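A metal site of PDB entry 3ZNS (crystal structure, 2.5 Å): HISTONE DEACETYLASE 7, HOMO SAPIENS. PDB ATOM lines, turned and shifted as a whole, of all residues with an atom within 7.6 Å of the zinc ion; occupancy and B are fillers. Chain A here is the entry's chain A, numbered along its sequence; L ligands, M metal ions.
A ring nitrogen (ND1) of His 229 lies close to a nitrogen (N3) of the ligand, at 3.4 Å.
A ring nitrogen (NE2) of His 190 sits at hydrogen-bond distance from a nitrogen (N2) of the ligand, at 3.3 Å.
The side-chain carboxylate of Asp 321 sits at hydrogen-bond distance from the backbone NH of Val 228 (2.8 Å).
The backbone NH (N) of Gly 361 sits at hydrogen-bond distance from the side-chain carboxylate (OD2) of Asp 227, 2.9 Å away.
The backbone NH (N) of Asp 227 lies within hydrogen-bond range of the side-chain carboxylate (OD1) of Asp 225, 3.3 Å away.
A ring nitrogen (NE2) of His 229 sits close to the backbone carbonyl oxygen (O) of Leu 330 (3.4 Å).
Three residues have an atom within 4 Å of the zinc ion: Asp 227, His 229 and Asp 321.
The zinc ion is bound by ND1 of His 229 (2.0 Å), OD2 of Asp 321 (2.0 Å) and OD1 of Asp 227 (2.0 Å).
The zinc ion has three donor atoms within binding distance.
Slightly farther from the zinc ion lies a fluorine (F3) of the ligand (2.7 Å).
Slightly farther from the zinc ion lies O1 of the ligand (2.7 Å).
Slightly farther from the zinc ion lies OD2 of Asp 227 (2.8 Å).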
ATOM      1  N   PRO A 187      -2.678   7.651  14.990  1.00  0.00           N
ATOM      2  CA  PRO A 187      -3.439   8.831  15.413  1.00  0.00           C
ATOM      3  C   PRO A 187      -4.813   8.460  16.011  1.00  0.00           C
ATOM      4  O   PRO A 187      -5.219   7.290  15.949  1.00  0.00           O
ATOM      5  CB  PRO A 187      -3.589   9.618  14.114  1.00  0.00           C
ATOM      6  CG  PRO A 187      -3.517   8.609  13.046  1.00  0.00           C
ATOM      7  CD  PRO A 187      -2.578   7.549  13.530  1.00  0.00           C
ATOM      8  N   HIS A 189      -7.882  11.184  16.531  1.00  0.00           N
ATOM      9  CA  HIS A 189      -9.042  12.096  16.508  1.00  0.00           C
ATOM     10  C   HIS A 189     -10.192  11.731  15.562  1.00  0.00           C
ATOM     11  O   HIS A 189     -11.274  12.312  15.672  1.00  0.00           O
ATOM     12  CB  HIS A 189      -8.583  13.551  16.305  1.00  0.00           C
ATOM     13  CG  HIS A 189      -8.091  13.860  14.915  1.00  0.00           C
ATOM     14  ND1 HIS A 189      -8.096  15.132  14.400  1.00  0.00           N
ATOM     15  CD2 HIS A 189      -7.590  13.059  13.940  1.00  0.00           C
ATOM     16  CE1 HIS A 189      -7.617  15.103  13.163  1.00  0.00           C
ATOM     17  NE2 HIS A 189      -7.306  13.853  12.866  1.00  0.00           N
ATOM     18  N   HIS A 190      -9.993  10.767  14.667  1.00  0.00           N
ATOM     19  CA  HIS A 190     -11.078  10.288  13.802  1.00  0.00           C
ATOM     20  C   HIS A 190     -11.885   9.139  14.417  1.00  0.00           C
ATOM     21  O   HIS A 190     -13.023   8.890  14.027  1.00  0.00           O
ATOM     22  CB  HIS A 190     -10.561   9.855  12.421  1.00  0.00           C
ATOM     23  CG  HIS A 190     -10.027  10.992  11.600  1.00  0.00           C
ATOM     24  ND1 HIS A 190     -10.687  12.193  11.451  1.00  0.00           N
ATOM     25  CD2 HIS A 190      -8.905  11.093  10.847  1.00  0.00           C
ATOM     26  CE1 HIS A 190      -9.983  12.984  10.654  1.00  0.00           C
ATOM     27  NE2 HIS A 190      -8.897  12.342  10.278  1.00  0.00           N
ATOM     28  N   GLY A 198     -10.137   6.384   9.362  1.00  0.00           N
ATOM     29  CA  GLY A 198      -9.118   7.400   9.047  1.00  0.00           C
ATOM     30  C   GLY A 198      -7.818   7.188   9.808  1.00  0.00           C
ATOM     31  O   GLY A 198      -7.304   8.116  10.429  1.00  0.00           O
ATOM     32  N   PHE A 199      -7.299   5.965   9.741  1.00  0.00           N
ATOM     33  CA  PHE A 199      -6.051   5.575  10.410  1.00  0.00           C
ATOM     34  C   PHE A 199      -6.133   5.580  11.951  1.00  0.00           C
ATOM     35  O   PHE A 199      -5.097   5.461  12.610  1.00  0.00           O
ATOM     36  CB  PHE A 199      -4.871   6.455   9.961  1.00  0.00           C
ATOM     37  CG  PHE A 199      -4.696   6.515   8.456  1.00  0.00           C
ATOM     38  CD1 PHE A 199      -3.966   5.539   7.787  1.00  0.00           C
ATOM     39  CD2 PHE A 199      -5.253   7.550   7.724  1.00  0.00           C
ATOM     40  CE1 PHE A 199      -3.793   5.602   6.403  1.00  0.00           C
ATOM     41  CE2 PHE A 199      -5.087   7.614   6.334  1.00  0.00           C
ATOM     42  CZ  PHE A 199      -4.357   6.642   5.681  1.00  0.00           C
ATOM     43  N   ASP A 225      -7.528  21.460  17.922  1.00  0.00           N
ATOM     44  CA  ASP A 225      -7.155  20.495  16.909  1.00  0.00           C
ATOM     45  C   ASP A 225      -6.763  21.252  15.635  1.00  0.00           C
ATOM     46  O   ASP A 225      -7.637  21.741  14.914  1.00  0.00           O
ATOM     47  CB  ASP A 225      -8.351  19.554  16.699  1.00  0.00           C
ATOM     48  CG  ASP A 225      -8.041  18.381  15.775  1.00  0.00           C
ATOM     49  OD1 ASP A 225      -7.177  18.513  14.885  1.00  0.00           O
ATOM     50  OD2 ASP A 225      -8.694  17.325  15.944  1.00  0.00           O
ATOM     51  N   TRP A 226      -5.464  21.377  15.370  1.00  0.00           N
ATOM     52  CA  TRP A 226      -4.985  22.098  14.176  1.00  0.00           C
ATOM     53  C   TRP A 226      -4.512  21.187  13.037  1.00  0.00           C
ATOM     54  O   TRP A 226      -3.961  21.651  12.044  1.00  0.00           O
ATOM     55  CB  TRP A 226      -3.913  23.143  14.535  1.00  0.00           C
ATOM     56  CG  TRP A 226      -2.631  22.621  15.106  1.00  0.00           C
ATOM     57  CD1 TRP A 226      -1.910  21.545  14.670  1.00  0.00           C
ATOM     58  CD2 TRP A 226      -1.888  23.178  16.206  1.00  0.00           C
ATOM     59  NE1 TRP A 226      -0.780  21.396  15.433  1.00  0.00           N
ATOM     60  CE2 TRP A 226      -0.745  22.382  16.387  1.00  0.00           C
ATOM     61  CE3 TRP A 226      -2.085  24.275  17.052  1.00  0.00           C
ATOM     62  CZ2 TRP A 226       0.203  22.644  17.371  1.00  0.00           C
ATOM     63  CZ3 TRP A 226      -1.146  24.538  18.030  1.00  0.00           C
ATOM     64  CH2 TRP A 226      -0.016  23.725  18.193  1.00  0.00           C
ATOM     65  N   ASP A 227      -4.720  19.878  13.192  1.00  0.00           N
ATOM     66  CA  ASP A 227      -4.591  18.940  12.092  1.00  0.00           C
ATOM     67  C   ASP A 227      -5.548  19.425  10.994  1.00  0.00           C
ATOM     68  O   ASP A 227      -6.617  19.965  11.299  1.00  0.00           O
ATOM     69  CB  ASP A 227      -4.969  17.530  12.581  1.00  0.00           C
ATOM     70  CG  ASP A 227      -4.764  16.455  11.509  1.00  0.00           C
ATOM     71  OD1 ASP A 227      -5.444  16.494  10.462  1.00  0.00           O
ATOM     72  OD2 ASP A 227      -3.935  15.546  11.742  1.00  0.00           O
ATOM     73  N   VAL A 228      -5.163  19.254   9.729  1.00  0.00           N
ATOM     74  CA  VAL A 228      -5.952  19.799   8.614  1.00  0.00           C
ATOM     75  C   VAL A 228      -7.299  19.091   8.439  1.00  0.00           C
ATOM     76  O   VAL A 228      -8.217  19.667   7.856  1.00  0.00           O
ATOM     77  CB  VAL A 228      -5.149  19.767   7.295  1.00  0.00           C
ATOM     78  CG1 VAL A 228      -5.127  18.345   6.722  1.00  0.00           C
ATOM     79  CG2 VAL A 228      -5.727  20.758   6.299  1.00  0.00           C
ATOM     80  N   HIS A 229      -7.434  17.867   8.946  1.00  0.00           N
ATOM     81  CA  HIS A 229      -8.711  17.138   8.926  1.00  0.00           C
ATOM     82  C   HIS A 229      -9.504  17.394  10.215  1.00  0.00           C
ATOM     83  O   HIS A 229      -8.908  17.528  11.283  1.00  0.00           O
ATOM     84  CB  HIS A 229      -8.485  15.643   8.792  1.00  0.00           C
ATOM     85  CG  HIS A 229      -7.607  15.269   7.640  1.00  0.00           C
ATOM     86  ND1 HIS A 229      -6.226  15.230   7.746  1.00  0.00           N
ATOM     87  CD2 HIS A 229      -7.904  14.947   6.362  1.00  0.00           C
ATOM     88  CE1 HIS A 229      -5.720  14.875   6.577  1.00  0.00           C
ATOM     89  NE2 HIS A 229      -6.713  14.704   5.717  1.00  0.00           N
ATOM     90  N   HIS A 230     -10.822  17.441  10.109  1.00  0.00           N
ATOM     91  CA  HIS A 230     -11.699  17.593  11.260  1.00  0.00           C
ATOM     92  C   HIS A 230     -11.624  16.370  12.175  1.00  0.00           C
ATOM     93  O   HIS A 230     -11.719  15.239  11.702  1.00  0.00           O
ATOM     94  CB  HIS A 230     -13.142  17.830  10.814  1.00  0.00           C
ATOM     95  CG  HIS A 230     -14.101  18.030  11.947  1.00  0.00           C
ATOM     96  ND1 HIS A 230     -15.119  17.152  12.229  1.00  0.00           N
ATOM     97  CD2 HIS A 230     -14.177  19.018  12.882  1.00  0.00           C
ATOM     98  CE1 HIS A 230     -15.794  17.586  13.284  1.00  0.00           C
ATOM     99  NE2 HIS A 230     -15.237  18.716  13.691  1.00  0.00           N
ATOM    100  N   PHE A 257     -14.052  17.097   1.923  1.00  0.00           N
ATOM    101  CA  PHE A 257     -12.708  16.770   2.372  1.00  0.00           C
ATOM    102  C   PHE A 257     -12.832  15.924   3.644  1.00  0.00           C
ATOM    103  O   PHE A 257     -13.623  16.241   4.517  1.00  0.00           O
ATOM    104  CB  PHE A 257     -11.908  18.042   2.642  1.00  0.00           C
ATOM    105  CG  PHE A 257     -10.436  17.812   2.884  1.00  0.00           C
ATOM    106  CD1 PHE A 257      -9.585  17.524   1.816  1.00  0.00           C
ATOM    107  CD2 PHE A 257      -9.907  17.877   4.166  1.00  0.00           C
ATOM    108  CE1 PHE A 257      -8.234  17.306   2.036  1.00  0.00           C
ATOM    109  CE2 PHE A 257      -8.555  17.659   4.386  1.00  0.00           C
ATOM    110  CZ  PHE A 257      -7.713  17.382   3.315  1.00  0.00           C
ATOM    111  N   PHE A 258     -12.048  14.846   3.728  1.00  0.00           N
ATOM    112  CA  PHE A 258     -12.208  13.890   4.830  1.00  0.00           C
ATOM    113  C   PHE A 258     -12.051  14.573   6.180  1.00  0.00           C
ATOM    114  O   PHE A 258     -11.165  15.404   6.339  1.00  0.00           O
ATOM    115  CB  PHE A 258     -11.202  12.731   4.704  1.00  0.00           C
ATOM    116  CG  PHE A 258     -11.447  11.604   5.677  1.00  0.00           C
ATOM    117  CD1 PHE A 258     -10.944  11.661   6.976  1.00  0.00           C
ATOM    118  CD2 PHE A 258     -12.207  10.497   5.310  1.00  0.00           C
ATOM    119  CE1 PHE A 258     -11.183  10.630   7.888  1.00  0.00           C
ATOM    120  CE2 PHE A 258     -12.447   9.461   6.205  1.00  0.00           C
ATOM    121  CZ  PHE A 258     -11.938   9.521   7.496  1.00  0.00           C
ATOM    122  N   GLY A 319      -1.745  17.658  14.621  1.00  0.00           N
ATOM    123  CA  GLY A 319      -1.399  17.138  13.308  1.00  0.00           C
ATOM    124  C   GLY A 319      -0.604  18.181  12.558  1.00  0.00           C
ATOM    125  O   GLY A 319      -0.801  19.381  12.763  1.00  0.00           O
ATOM    126  N   PHE A 320       0.293  17.742  11.676  1.00  0.00           N
ATOM    127  CA  PHE A 320       1.105  18.662  10.886  1.00  0.00           C
ATOM    128  C   PHE A 320       0.902  18.490   9.385  1.00  0.00           C
ATOM    129  O   PHE A 320       1.794  18.773   8.597  1.00  0.00           O
ATOM    130  CB  PHE A 320       2.573  18.500  11.277  1.00  0.00           C
ATOM    131  CG  PHE A 320       2.837  18.827  12.719  1.00  0.00           C
ATOM    132  CD1 PHE A 320       2.690  20.117  13.189  1.00  0.00           C
ATOM    133  CD2 PHE A 320       3.217  17.833  13.611  1.00  0.00           C
ATOM    134  CE1 PHE A 320       2.929  20.428  14.510  1.00  0.00           C
ATOM    135  CE2 PHE A 320       3.466  18.133  14.935  1.00  0.00           C
ATOM    136  CZ  PHE A 320       3.312  19.441  15.382  1.00  0.00           C
ATOM    137  N   ASP A 321      -0.299  18.060   9.003  1.00  0.00           N
ATOM    138  CA  ASP A 321      -0.657  17.880   7.591  1.00  0.00           C
ATOM    139  C   ASP A 321      -1.217  19.160   6.949  1.00  0.00           C
ATOM    140  O   ASP A 321      -1.612  19.140   5.779  1.00  0.00           O
ATOM    141  CB  ASP A 321      -1.597  16.679   7.402  1.00  0.00           C
ATOM    142  CG  ASP A 321      -2.719  16.626   8.432  1.00  0.00           C
ATOM    143  OD1 ASP A 321      -2.981  17.654   9.102  1.00  0.00           O
ATOM    144  OD2 ASP A 321      -3.335  15.549   8.581  1.00  0.00           O
ATOM    145  N   ALA A 322      -1.272  20.253   7.704  1.00  0.00           N
ATOM    146  CA  ALA A 322      -1.530  21.582   7.135  1.00  0.00           C
ATOM    147  C   ALA A 322      -0.206  22.219   6.708  1.00  0.00           C
ATOM    148  O   ALA A 322      -0.194  23.278   6.073  1.00  0.00           O
ATOM    149  CB  ALA A 322      -2.254  22.482   8.138  1.00  0.00           C
ATOM    150  N   LEU A 330      -4.218  15.446   0.335  1.00  0.00           N
ATOM    151  CA  LEU A 330      -3.821  15.115   1.704  1.00  0.00           C
ATOM    152  C   LEU A 330      -3.944  16.347   2.587  1.00  0.00           C
ATOM    153  O   LEU A 330      -4.326  16.231   3.757  1.00  0.00           O
ATOM    154  CB  LEU A 330      -2.380  14.597   1.744  1.00  0.00           C
ATOM    155  CG  LEU A 330      -1.781  14.368   3.142  1.00  0.00           C
ATOM    156  CD1 LEU A 330      -2.745  13.624   4.077  1.00  0.00           C
ATOM    157  CD2 LEU A 330      -0.466  13.607   3.029  1.00  0.00           C
ATOM    158  N   GLU A 360      -1.043  13.806  15.725  1.00  0.00           N
ATOM    159  CA  GLU A 360      -2.116  13.160  14.987  1.00  0.00           C
ATOM    160  C   GLU A 360      -1.528  12.866  13.599  1.00  0.00           C
ATOM    161  O   GLU A 360      -0.725  11.959  13.463  1.00  0.00           O
ATOM    162  CB  GLU A 360      -3.364  14.039  14.960  1.00  0.00           C
ATOM    163  CG  GLU A 360      -3.941  14.349  16.336  1.00  0.00           C
ATOM    164  CD  GLU A 360      -4.848  13.254  16.907  1.00  0.00           C
ATOM    165  OE1 GLU A 360      -5.005  12.183  16.291  1.00  0.00           O
ATOM    166  OE2 GLU A 360      -5.420  13.488  17.997  1.00  0.00           O
ATOM    167  N   GLY A 361      -1.894  13.666  12.593  1.00  0.00           N
ATOM    168  CA  GLY A 361      -1.485  13.409  11.216  1.00  0.00           C
ATOM    169  C   GLY A 361      -0.209  14.136  10.817  1.00  0.00           C
ATOM    170  O   GLY A 361       0.423  14.799  11.645  1.00  0.00           O
ATOM    171  N   GLY A 362       0.142  14.029   9.539  1.00  0.00           N
ATOM    172  CA  GLY A 362       1.378  14.565   8.998  1.00  0.00           C
ATOM    173  C   GLY A 362       2.202  13.446   8.383  1.00  0.00           C
ATOM    174  O   GLY A 362       2.505  12.469   9.060  1.00  0.00           O
HETATM  175  C1  LIG L   1      -3.159   6.052  -0.606  1.00  0.00           C
HETATM  176  N1  LIG L   1      -4.399   6.802  -0.882  1.00  0.00           N
HETATM  177  F1  LIG L   1      -3.857  11.298  11.238  1.00  0.00           F
HETATM  178  C2  LIG L   1      -5.053  11.778  10.931  1.00  0.00           C
HETATM  179  F2  LIG L   1      -5.966  11.040  11.546  1.00  0.00           F
HETATM  180  F3  LIG L   1      -5.169  13.051  11.272  1.00  0.00           F
HETATM  181  C3  LIG L   1      -5.254  11.728   9.444  1.00  0.00           C
HETATM  182  N2  LIG L   1      -6.209  11.088   8.802  1.00  0.00           N
HETATM  183  C4  LIG L   1      -6.039  11.307   7.428  1.00  0.00           C
HETATM  184  N3  LIG L   1      -4.974  12.066   7.267  1.00  0.00           N
HETATM  185  O1  LIG L   1      -4.444  12.365   8.516  1.00  0.00           O
HETATM  186  C5  LIG L   1      -6.874  10.751   6.351  1.00  0.00           C
HETATM  187  C6  LIG L   1      -8.061  10.077   6.655  1.00  0.00           C
HETATM  188  C7  LIG L   1      -8.831   9.540   5.610  1.00  0.00           C
HETATM  189  C8  LIG L   1      -8.413   9.683   4.279  1.00  0.00           C
HETATM  190  C9  LIG L   1      -7.228  10.366   3.978  1.00  0.00           C
HETATM  191  C10 LIG L   1      -6.448  10.892   5.025  1.00  0.00           C
HETATM  192  C11 LIG L   1      -6.777  10.491   2.584  1.00  0.00           C
HETATM  193  O2  LIG L   1      -7.593  10.689   1.674  1.00  0.00           O
HETATM  194  N4  LIG L   1      -5.478  10.326   2.327  1.00  0.00           N
HETATM  195  C12 LIG L   1      -4.923  10.233   0.961  1.00  0.00           C
HETATM  196  C13 LIG L   1      -3.861   9.118   0.885  1.00  0.00           C
HETATM  197  C14 LIG L   1      -3.292   9.028  -0.549  1.00  0.00           C
HETATM  198  C15 LIG L   1      -4.109   8.111  -1.485  1.00  0.00           C
HETATM  199  C16 LIG L   1      -5.199   6.974   0.337  1.00  0.00           C
HETATM  200  C17 LIG L   1      -4.443   7.777   1.405  1.00  0.00           C
HETATM  201  C18 LIG L   1      -2.748   9.530   1.837  1.00  0.00           C
HETATM  202  N5  LIG L   1      -2.764   9.476   3.162  1.00  0.00           N
HETATM  203  C19 LIG L   1      -1.610   9.907   3.844  1.00  0.00           C
HETATM  204  C20 LIG L   1      -0.597  10.331   3.065  1.00  0.00           C
HETATM  205  S1  LIG L   1      -1.165  10.164   1.398  1.00  0.00           S
HETATM  206  C21 LIG L   1      -1.530   9.898   5.331  1.00  0.00           C
HETATM  207  C22 LIG L   1      -0.283   9.893   5.992  1.00  0.00           C
HETATM  208  C23 LIG L   1      -0.224   9.877   7.392  1.00  0.00           C
HETATM  209  C24 LIG L   1      -1.400   9.884   8.149  1.00  0.00           C
HETATM  210  C25 LIG L   1      -2.639   9.888   7.494  1.00  0.00           C
HETATM  211  C26 LIG L   1      -2.701   9.891   6.099  1.00  0.00           C
HETATM  212 ZN    ZN M   1      -5.074  14.900   9.294  1.00  0.00          ZN
